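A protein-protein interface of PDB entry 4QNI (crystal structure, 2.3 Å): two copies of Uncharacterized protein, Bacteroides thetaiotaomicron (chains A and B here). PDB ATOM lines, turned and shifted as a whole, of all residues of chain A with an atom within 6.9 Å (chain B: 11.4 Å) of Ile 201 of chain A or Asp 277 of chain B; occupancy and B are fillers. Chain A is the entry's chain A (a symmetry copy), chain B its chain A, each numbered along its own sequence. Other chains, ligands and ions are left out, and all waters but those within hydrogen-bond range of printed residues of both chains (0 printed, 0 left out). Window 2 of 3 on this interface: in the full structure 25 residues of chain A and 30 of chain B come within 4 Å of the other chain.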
ATOM      1  N   GLY A 177      -8.603  23.926  16.954  1.00  0.00           N
ATOM      2  CA  GLY A 177      -7.623  23.500  17.952  1.00  0.00           C
ATOM      3  C   GLY A 177      -6.206  23.414  17.389  1.00  0.00           C
ATOM      4  O   GLY A 177      -5.293  22.954  18.067  1.00  0.00           O
ATOM      5  N   ILE A 180      -3.352  24.780  19.513  1.00  0.00           N
ATOM      6  CA  ILE A 180      -3.242  24.240  20.860  1.00  0.00           C
ATOM      7  C   ILE A 180      -2.443  22.971  20.820  1.00  0.00           C
ATOM      8  O   ILE A 180      -2.784  22.076  20.044  1.00  0.00           O
ATOM      9  CB  ILE A 180      -4.639  23.991  21.514  1.00  0.00           C
ATOM     10  CG1 ILE A 180      -5.388  25.312  21.816  1.00  0.00           C
ATOM     11  CG2 ILE A 180      -4.505  23.130  22.788  1.00  0.00           C
ATOM     12  CD1 ILE A 180      -4.737  26.211  22.878  1.00  0.00           C
ATOM     13  N   THR A 181      -1.412  22.861  21.673  1.00  0.00           N
ATOM     14  CA  THR A 181      -0.670  21.609  21.786  1.00  0.00           C
ATOM     15  C   THR A 181      -1.081  20.925  23.093  1.00  0.00           C
ATOM     16  O   THR A 181      -1.499  21.599  24.057  1.00  0.00           O
ATOM     17  CB  THR A 181       0.859  21.766  21.672  1.00  0.00           C
ATOM     18  OG1 THR A 181       1.369  22.613  22.705  1.00  0.00           O
ATOM     19  CG2 THR A 181       1.307  22.225  20.297  1.00  0.00           C
ATOM     20  N   ASN A 182      -1.013  19.583  23.091  1.00  0.00           N
ATOM     21  CA  ASN A 182      -1.264  18.729  24.247  1.00  0.00           C
ATOM     22  C   ASN A 182      -0.047  17.846  24.426  1.00  0.00           C
ATOM     23  O   ASN A 182       0.217  16.973  23.591  1.00  0.00           O
ATOM     24  CB  ASN A 182      -2.544  17.892  24.071  1.00  0.00           C
ATOM     25  CG  ASN A 182      -3.813  18.694  24.048  1.00  0.00           C
ATOM     26  OD1 ASN A 182      -4.401  18.975  25.076  1.00  0.00           O
ATOM     27  ND2 ASN A 182      -4.263  19.088  22.881  1.00  0.00           N
ATOM     28  N   LYS A 183       0.737  18.115  25.468  1.00  0.00           N
ATOM     29  CA  LYS A 183       1.939  17.347  25.764  1.00  0.00           C
ATOM     30  C   LYS A 183       1.759  16.655  27.107  1.00  0.00           C
ATOM     31  O   LYS A 183       0.960  17.126  27.905  1.00  0.00           O
ATOM     32  CB  LYS A 183       3.182  18.262  25.755  1.00  0.00           C
ATOM     33  CG  LYS A 183       3.546  18.750  24.358  1.00  0.00           C
ATOM     34  CD  LYS A 183       4.534  19.883  24.413  1.00  0.00           C
ATOM     35  CE  LYS A 183       5.040  20.252  23.041  1.00  0.00           C
ATOM     36  NZ  LYS A 183       6.521  20.361  23.029  1.00  0.00           N
ATOM     37  N   VAL A 184       2.460  15.526  27.341  1.00  0.00           N
ATOM     38  CA  VAL A 184       2.375  14.756  28.574  1.00  0.00           C
ATOM     39  C   VAL A 184       3.587  15.081  29.460  1.00  0.00           C
ATOM     40  O   VAL A 184       4.733  14.985  29.008  1.00  0.00           O
ATOM     41  CB  VAL A 184       2.267  13.223  28.277  1.00  0.00           C
ATOM     42  CG1 VAL A 184       2.328  12.378  29.556  1.00  0.00           C
ATOM     43  CG2 VAL A 184       1.009  12.890  27.474  1.00  0.00           C
ATOM     44  N   THR A 197       6.704  15.573  26.861  1.00  0.00           N
ATOM     45  CA  THR A 197       6.839  14.886  25.592  1.00  0.00           C
ATOM     46  C   THR A 197       7.040  15.904  24.505  1.00  0.00           C
ATOM     47  O   THR A 197       6.524  17.028  24.584  1.00  0.00           O
ATOM     48  CB  THR A 197       5.638  14.013  25.302  1.00  0.00           C
ATOM     49  OG1 THR A 197       4.463  14.826  25.280  1.00  0.00           O
ATOM     50  CG2 THR A 197       5.509  12.880  26.291  1.00  0.00           C
ATOM     51  N   GLU A 199       6.338  15.254  21.102  1.00  0.00           N
ATOM     52  CA  GLU A 199       5.167  15.150  20.238  1.00  0.00           C
ATOM     53  C   GLU A 199       3.916  15.652  20.951  1.00  0.00           C
ATOM     54  O   GLU A 199       3.813  15.564  22.179  1.00  0.00           O
ATOM     55  CB  GLU A 199       4.963  13.707  19.748  1.00  0.00           C
ATOM     56  N   SER A 200       2.971  16.178  20.159  1.00  0.00           N
ATOM     57  CA  SER A 200       1.710  16.713  20.639  1.00  0.00           C
ATOM     58  C   SER A 200       0.506  16.006  19.994  1.00  0.00           C
ATOM     59  O   SER A 200       0.559  15.578  18.839  1.00  0.00           O
ATOM     60  CB  SER A 200       1.646  18.220  20.374  1.00  0.00           C
ATOM     61  OG  SER A 200       0.324  18.707  20.193  1.00  0.00           O
ATOM     62  N   ILE A 201      -0.588  15.934  20.756  1.00  0.00           N
ATOM     63  CA  ILE A 201      -1.881  15.414  20.323  1.00  0.00           C
ATOM     64  C   ILE A 201      -2.694  16.644  19.927  1.00  0.00           C
ATOM     65  O   ILE A 201      -2.911  17.528  20.767  1.00  0.00           O
ATOM     66  CB  ILE A 201      -2.569  14.548  21.427  1.00  0.00           C
ATOM     67  CG1 ILE A 201      -1.627  13.434  21.958  1.00  0.00           C
ATOM     68  CG2 ILE A 201      -3.899  13.968  20.926  1.00  0.00           C
ATOM     69  CD1 ILE A 201      -1.870  13.011  23.429  1.00  0.00           C
ATOM     70  N   THR A 202      -3.077  16.754  18.648  1.00  0.00           N
ATOM     71  CA  THR A 202      -3.813  17.946  18.273  1.00  0.00           C
ATOM     72  C   THR A 202      -5.267  17.611  17.974  1.00  0.00           C
ATOM     73  O   THR A 202      -5.572  16.771  17.116  1.00  0.00           O
ATOM     74  CB  THR A 202      -3.134  18.735  17.140  1.00  0.00           C
ATOM     75  OG1 THR A 202      -1.785  19.043  17.539  1.00  0.00           O
ATOM     76  CG2 THR A 202      -3.875  20.053  16.816  1.00  0.00           C
ATOM     77  N   LYS A 203      -6.150  18.273  18.744  1.00  0.00           N
ATOM     78  CA  LYS A 203      -7.596  18.291  18.590  1.00  0.00           C
ATOM     79  C   LYS A 203      -7.870  19.366  17.565  1.00  0.00           C
ATOM     80  O   LYS A 203      -7.674  20.538  17.881  1.00  0.00           O
ATOM     81  CB  LYS A 203      -8.278  18.629  19.936  1.00  0.00           C
ATOM     82  CG  LYS A 203      -8.654  17.438  20.791  1.00  0.00           C
ATOM     83  CD  LYS A 203      -9.945  17.708  21.561  1.00  0.00           C
ATOM     84  CE  LYS A 203     -11.182  17.269  20.806  1.00  0.00           C
ATOM     85  NZ  LYS A 203     -11.252  15.781  20.675  1.00  0.00           N
ATOM     86  N   ILE A 222      -7.642  17.059  25.503  1.00  0.00           N
ATOM     87  CA  ILE A 222      -8.131  16.087  24.513  1.00  0.00           C
ATOM     88  C   ILE A 222      -9.506  15.536  24.850  1.00  0.00           C
ATOM     89  O   ILE A 222     -10.108  14.867  24.004  1.00  0.00           O
ATOM     90  CB  ILE A 222      -7.118  14.946  24.305  1.00  0.00           C
ATOM     91  CG1 ILE A 222      -6.803  14.236  25.633  1.00  0.00           C
ATOM     92  CG2 ILE A 222      -5.862  15.495  23.639  1.00  0.00           C
ATOM     93  CD1 ILE A 222      -6.199  13.007  25.458  1.00  0.00           C
ATOM     94  N   TYR A 227     -16.546  11.517  25.675  1.00  0.00           N
ATOM     95  CA  TYR A 227     -15.951  10.952  26.895  1.00  0.00           C
ATOM     96  C   TYR A 227     -17.063  10.757  27.910  1.00  0.00           C
ATOM     97  O   TYR A 227     -17.782  11.712  28.227  1.00  0.00           O
ATOM     98  CB  TYR A 227     -14.855  11.885  27.474  1.00  0.00           C
ATOM     99  CG  TYR A 227     -13.508  11.782  26.789  1.00  0.00           C
ATOM    100  CD1 TYR A 227     -13.379  12.011  25.420  1.00  0.00           C
ATOM    101  CD2 TYR A 227     -12.356  11.461  27.511  1.00  0.00           C
ATOM    102  CE1 TYR A 227     -12.148  11.881  24.779  1.00  0.00           C
ATOM    103  CE2 TYR A 227     -11.109  11.376  26.887  1.00  0.00           C
ATOM    104  CZ  TYR A 227     -11.012  11.579  25.518  1.00  0.00           C
ATOM    105  OH  TYR A 227      -9.803  11.492  24.880  1.00  0.00           O
ATOM    106  N   TYR A 308      -1.379  16.222  31.562  1.00  0.00           N
ATOM    107  CA  TYR A 308      -1.257  16.952  30.304  1.00  0.00           C
ATOM    108  C   TYR A 308      -0.921  18.397  30.500  1.00  0.00           C
ATOM    109  O   TYR A 308      -1.382  19.011  31.461  1.00  0.00           O
ATOM    110  CB  TYR A 308      -2.562  16.879  29.509  1.00  0.00           C
ATOM    111  CG  TYR A 308      -2.814  15.530  28.887  1.00  0.00           C
ATOM    112  CD1 TYR A 308      -2.197  15.167  27.696  1.00  0.00           C
ATOM    113  CD2 TYR A 308      -3.688  14.623  29.478  1.00  0.00           C
ATOM    114  CE1 TYR A 308      -2.442  13.936  27.102  1.00  0.00           C
ATOM    115  CE2 TYR A 308      -3.937  13.383  28.895  1.00  0.00           C
ATOM    116  CZ  TYR A 308      -3.311  13.043  27.704  1.00  0.00           C
ATOM    117  OH  TYR A 308      -3.536  11.829  27.100  1.00  0.00           O
ATOM    118  N   SER B 273      -0.108  -4.830  25.123  1.00  0.00           N
ATOM    119  CA  SER B 273      -0.981  -3.661  25.135  1.00  0.00           C
ATOM    120  C   SER B 273      -0.266  -2.344  24.857  1.00  0.00           C
ATOM    121  O   SER B 273       0.930  -2.174  25.117  1.00  0.00           O
ATOM    122  CB  SER B 273      -1.681  -3.542  26.481  1.00  0.00           C
ATOM    123  OG  SER B 273      -2.883  -4.288  26.448  1.00  0.00           O
ATOM    124  N   SER B 274      -1.049  -1.398  24.339  1.00  0.00           N
ATOM    125  CA  SER B 274      -0.652  -0.035  24.020  1.00  0.00           C
ATOM    126  C   SER B 274      -1.872   0.866  24.096  1.00  0.00           C
ATOM    127  O   SER B 274      -2.963   0.485  23.662  1.00  0.00           O
ATOM    128  CB  SER B 274       0.001   0.039  22.642  1.00  0.00           C
ATOM    129  OG  SER B 274       0.241   1.390  22.280  1.00  0.00           O
ATOM    130  N   MET B 275      -1.681   2.045  24.677  1.00  0.00           N
ATOM    131  CA  MET B 275      -2.688   3.084  24.831  1.00  0.00           C
ATOM    132  C   MET B 275      -2.819   3.854  23.523  1.00  0.00           C
ATOM    133  O   MET B 275      -1.822   4.023  22.804  1.00  0.00           O
ATOM    134  CB  MET B 275      -2.288   4.038  25.975  1.00  0.00           C
ATOM    135  CG  MET B 275      -3.400   4.283  26.975  1.00  0.00           C
ATOM    136  N   ASP B 276      -4.046   4.305  23.198  1.00  0.00           N
ATOM    137  CA  ASP B 276      -4.264   5.120  22.007  1.00  0.00           C
ATOM    138  C   ASP B 276      -3.784   6.547  22.297  1.00  0.00           C
ATOM    139  O   ASP B 276      -3.843   6.985  23.457  1.00  0.00           O
ATOM    140  CB  ASP B 276      -5.735   5.110  21.591  1.00  0.00           C
ATOM    141  CG  ASP B 276      -5.980   5.748  20.242  1.00  0.00           C
ATOM    142  OD1 ASP B 276      -5.606   5.136  19.224  1.00  0.00           O
ATOM    143  OD2 ASP B 276      -6.572   6.853  20.206  1.00  0.00           O
ATOM    144  N   ASP B 277      -3.277   7.257  21.264  1.00  0.00           N
ATOM    145  CA  ASP B 277      -2.782   8.638  21.436  1.00  0.00           C
ATOM    146  C   ASP B 277      -3.943   9.610  21.650  1.00  0.00           C
ATOM    147  O   ASP B 277      -3.944  10.382  22.624  1.00  0.00           O
ATOM    148  CB  ASP B 277      -1.919   9.074  20.234  1.00  0.00           C
ATOM    149  N   ALA B 278      -4.942   9.533  20.741  1.00  0.00           N
ATOM    150  CA  ALA B 278      -6.141  10.362  20.731  1.00  0.00           C
ATOM    151  C   ALA B 278      -7.048  10.084  21.934  1.00  0.00           C
ATOM    152  O   ALA B 278      -7.339  11.018  22.685  1.00  0.00           O
ATOM    153  CB  ALA B 278      -6.910  10.138  19.436  1.00  0.00           C
ATOM    154  N   LYS B 279      -7.490   8.808  22.113  1.00  0.00           N
ATOM    155  CA  LYS B 279      -8.381   8.401  23.204  1.00  0.00           C
ATOM    156  C   LYS B 279      -7.567   7.601  24.244  1.00  0.00           C
ATOM    157  O   LYS B 279      -7.447   6.385  24.101  1.00  0.00           O
ATOM    158  CB  LYS B 279      -9.602   7.596  22.681  1.00  0.00           C
ATOM    159  CG  LYS B 279     -10.252   8.110  21.395  1.00  0.00           C
ATOM    160  CD  LYS B 279     -11.551   7.352  21.055  1.00  0.00           C
ATOM    161  CE  LYS B 279     -11.515   6.537  19.775  1.00  0.00           C
ATOM    162  NZ  LYS B 279     -12.729   5.672  19.624  1.00  0.00           N
ATOM    163  N   PRO B 280      -7.002   8.236  25.303  1.00  0.00           N
ATOM    164  CA  PRO B 280      -6.187   7.470  26.270  1.00  0.00           C
ATOM    165  C   PRO B 280      -6.972   6.417  27.064  1.00  0.00           C
ATOM    166  O   PRO B 280      -6.351   5.602  27.730  1.00  0.00           O
ATOM    167  CB  PRO B 280      -5.583   8.546  27.181  1.00  0.00           C
ATOM    168  CG  PRO B 280      -6.469   9.699  27.039  1.00  0.00           C
ATOM    169  CD  PRO B 280      -7.030   9.667  25.651  1.00  0.00           C
ATOM    170  N   TYR B 281      -8.310   6.395  26.965  1.00  0.00           N
ATOM    171  CA  TYR B 281      -9.120   5.343  27.608  1.00  0.00           C
ATOM    172  C   TYR B 281      -9.202   4.097  26.721  1.00  0.00           C
ATOM    173  O   TYR B 281      -9.735   3.079  27.146  1.00  0.00           O
ATOM    174  CB  TYR B 281     -10.537   5.831  27.935  1.00  0.00           C
ATOM    175  CG  TYR B 281     -11.294   6.364  26.745  1.00  0.00           C
ATOM    176  CD1 TYR B 281     -11.870   5.501  25.818  1.00  0.00           C
ATOM    177  CD2 TYR B 281     -11.466   7.732  26.560  1.00  0.00           C
ATOM    178  CE1 TYR B 281     -12.574   5.985  24.720  1.00  0.00           C
ATOM    179  CE2 TYR B 281     -12.199   8.227  25.484  1.00  0.00           C
ATOM    180  CZ  TYR B 281     -12.755   7.348  24.569  1.00  0.00           C
ATOM    181  OH  TYR B 281     -13.506   7.813  23.518  1.00  0.00           O
ATOM    182  N   LEU B 282      -8.748   4.209  25.474  1.00  0.00           N
ATOM    183  CA  LEU B 282      -8.797   3.136  24.500  1.00  0.00           C
ATOM    184  C   LEU B 282      -7.480   2.362  24.525  1.00  0.00           C
ATOM    185  O   LEU B 282      -6.398   2.938  24.456  1.00  0.00           O
ATOM    186  CB  LEU B 282      -9.110   3.712  23.115  1.00  0.00           C
ATOM    187  CG  LEU B 282      -9.274   2.732  21.960  1.00  0.00           C
ATOM    188  CD1 LEU B 282     -10.574   1.938  22.078  1.00  0.00           C
ATOM    189  CD2 LEU B 282      -9.187   3.471  20.620  1.00  0.00           C
ATOM    190  N   GLU B 283      -7.588   1.048  24.676  1.00  0.00           N
ATOM    191  CA  GLU B 283      -6.442   0.162  24.757  1.00  0.00           C
ATOM    192  C   GLU B 283      -6.383  -0.722  23.504  1.00  0.00           C
ATOM    193  O   GLU B 283      -7.379  -1.339  23.133  1.00  0.00           O
ATOM    194  CB  GLU B 283      -6.561  -0.672  26.048  1.00  0.00           C
ATOM    195  CG  GLU B 283      -5.591  -1.835  26.193  1.00  0.00           C
ATOM    196  CD  GLU B 283      -5.847  -2.700  27.415  1.00  0.00           C
ATOM    197  OE1 GLU B 283      -7.026  -3.015  27.695  1.00  0.00           O
ATOM    198  OE2 GLU B 283      -4.863  -3.059  28.101  1.00  0.00           O
ATOM    199  N   HIS B 284      -5.211  -0.756  22.861  1.00  0.00           N
ATOM    200  CA  HIS B 284      -4.937  -1.620  21.719  1.00  0.00           C
ATOM    201  C   HIS B 284      -4.275  -2.874  22.258  1.00  0.00           C
ATOM    202  O   HIS B 284      -3.190  -2.778  22.844  1.00  0.00           O
ATOM    203  CB  HIS B 284      -4.018  -0.922  20.695  1.00  0.00           C
ATOM    204  CG  HIS B 284      -4.534   0.386  20.184  1.00  0.00           C
ATOM    205  ND1 HIS B 284      -5.613   0.452  19.314  1.00  0.00           N
ATOM    206  CD2 HIS B 284      -4.086   1.637  20.414  1.00  0.00           C
ATOM    207  CE1 HIS B 284      -5.794   1.732  19.063  1.00  0.00           C
ATOM    208  NE2 HIS B 284      -4.894   2.482  19.692  1.00  0.00           N
ATOM    209  N   TYR B 286      -2.768  -6.637  21.435  1.00  0.00           N
ATOM    210  CA  TYR B 286      -2.182  -7.335  20.304  1.00  0.00           C
ATOM    211  C   TYR B 286      -1.886  -8.772  20.599  1.00  0.00           C
ATOM    212  O   TYR B 286      -1.414  -9.091  21.686  1.00  0.00           O
ATOM    213  CB  TYR B 286      -0.877  -6.644  19.877  1.00  0.00           C
ATOM    214  CG  TYR B 286      -1.067  -5.192  19.505  1.00  0.00           C
ATOM    215  CD1 TYR B 286      -1.650  -4.832  18.291  1.00  0.00           C
ATOM    216  CD2 TYR B 286      -0.672  -4.172  20.365  1.00  0.00           C
ATOM    217  CE1 TYR B 286      -1.799  -3.496  17.926  1.00  0.00           C
ATOM    218  CE2 TYR B 286      -0.840  -2.830  20.021  1.00  0.00           C
ATOM    219  CZ  TYR B 286      -1.398  -2.498  18.796  1.00  0.00           C
ATOM    220  OH  TYR B 286      -1.569  -1.190  18.425  1.00  0.00           O
ATOM    221  N   ASP B 319      -9.355  -3.519  19.911  1.00  0.00           N
ATOM    222  CA  ASP B 319      -9.491  -2.272  20.640  1.00  0.00           C
ATOM    223  C   ASP B 319     -10.463  -2.438  21.743  1.00  0.00           C
ATOM    224  O   ASP B 319     -11.601  -2.855  21.521  1.00  0.00           O
ATOM    225  CB  ASP B 319      -9.887  -1.121  19.708  1.00  0.00           C
ATOM    226  CG  ASP B 319      -8.873  -0.922  18.599  1.00  0.00           C
ATOM    227  OD1 ASP B 319      -7.658  -0.869  18.908  1.00  0.00           O
ATOM    228  OD2 ASP B 319      -9.278  -0.949  17.416  1.00  0.00           O
ATOM    229  N   ILE B 320      -9.992  -2.139  22.955  1.00  0.00           N
ATOM    230  CA  ILE B 320     -10.744  -2.245  24.193  1.00  0.00           C
ATOM    231  C   ILE B 320     -10.990  -0.854  24.715  1.00  0.00           C
ATOM    232  O   ILE B 320     -10.049  -0.140  25.051  1.00  0.00           O
ATOM    233  CB  ILE B 320      -9.999  -3.133  25.240  1.00  0.00           C
ATOM    234  CG1 ILE B 320      -9.371  -4.439  24.644  1.00  0.00           C
ATOM    235  CG2 ILE B 320     -10.841  -3.380  26.494  1.00  0.00           C
ATOM    236  CD1 ILE B 320     -10.280  -5.497  24.115  1.00  0.00           C
ATOM    237  N   GLU B 332     -14.273  -2.955  20.770  1.00  0.00           N
ATOM    238  CA  GLU B 332     -14.716  -2.168  19.619  1.00  0.00           C
ATOM    239  C   GLU B 332     -14.438  -2.990  18.370  1.00  0.00           C
ATOM    240  O   GLU B 332     -13.418  -2.806  17.698  1.00  0.00           O
ATOM    241  CB  GLU B 332     -14.041  -0.784  19.576  1.00  0.00           C
ATOM    242  CG  GLU B 332     -14.529   0.153  20.665  1.00  0.00           C
ATOM    243  CD  GLU B 332     -14.057   1.593  20.588  1.00  0.00           C
ATOM    244  OE1 GLU B 332     -13.087   1.876  19.845  1.00  0.00           O
ATOM    245  OE2 GLU B 332     -14.666   2.444  21.278  1.00  0.00           O
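O of Ala 278 of chain B sits at hydrogen-bond distance from OH of Tyr 227 of chain A, 3.3 Å away.
The side-chain carboxylate (OD2) of Asp 276 of chain B sits at hydrogen-bond distance from the backbone NH (N) of Ala 278 of chain B (3.2 Å).
The side-chain carboxylate (OD2) of Asp 276 of chain B lies within hydrogen-bond range of the backbone NH (N) of Lys 279 of chain B (2.9 Å).
The side-chain amino group of Lys 279 of chain B lies within salt-bridge range of the side-chain carboxylate of Glu 332 of chain B, at 3.8 Å.
The backbone carbonyl oxygen (O) of Ile 201 of chain A lies within hydrogen-bond range of the side-chain amide nitrogen (ND2) of Asn 182 of chain A (3.0 Å).
The backbone carbonyl oxygen (O) of Ile 222 of chain A sits close to the side-chain hydroxyl (OH) of Tyr 227 of chain A (3.5 Å).
Asp 277 of chain B touches Ile 201 of chain A.
CD1 of Ile 222 of chain A touches O of Ala 278 of chain B, at 3.6 Å.
Ile 222 of chain A touches Pro 280 of chain B.
Lys 279 of chain B touches Tyr 227 of chain A.
Tyr 227 of chain A touches Pro 280 of chain B.
Tyr 227 of chain A touches Tyr 281 of chain B (CZ to CE2, 3.6 Å).
CG of Pro 280 of chain B touches OH of Tyr 308 of chain A, 3.6 Å away.
Ile 201 of chain A touches just one residue of chain B: Asp 277 (3.4 Å).
Asp 277 of chain B touches just one residue of chain A: Ile 201 (3.4 Å).
No residue of chain B comes within 4 Å of Thr 181 of chain A.
No residue of chain B comes within 4 Å of Asn 182 of chain A.
No residue of chain B comes within 4 Å of Glu 199 of chain A.
Ser 200 of chain A touches none of the printed residues of chain B.
Of the printed residues of chain A, Ala 278 of chain B touches Ile 222 and Tyr 227.
Printed residues of chain A within 4 Å of Pro 280 of chain B: Ile 222 (3.4 Å), Tyr 227 (3.4 Å) and Tyr 308 (3.6 Å).
Of the printed residues of chain A, Lys 279 of chain B touches Tyr 227.
Of the printed residues of chain A, Tyr 281 of chain B touches Tyr 227.
Glu 332 of chain B touches none of the printed residues of chain A.
Thr 197 of chain A touches none of the printed residues of chain B.
The nearest residue of chain B that does not touch Ile 201 of chain A is Ala 278 of chain B (4.3 Å).
The nearest residue of chain A that does not touch Asp 277 of chain B is Ile 222 of chain A (4.5 Å).
Of the 15 printed residues of chain A, 4 touch a printed residue of chain B.
Printed residues of chain A that touch a printed residue of chain B: Ile 201, Ile 222, Tyr 227 and Tyr 308.
Of the 16 printed residues of chain B, 5 touch a printed residue of chain A.
Printed residues of chain B that touch a printed residue of chain A: Asp 277, Ala 278, Lys 279, Pro 280 and Tyr 281.
Hydrophobic or aromatic side chains of chain B within 4 Å of the printed part of chain A: Pro 280 and Tyr 281.
Among the printed residues, 8 pairs touch across the chains.
No position is printed for both chains.
Of the 8 pairs that touch across the chains among the printed residues, none has its exchanged pair printed and touching as well.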
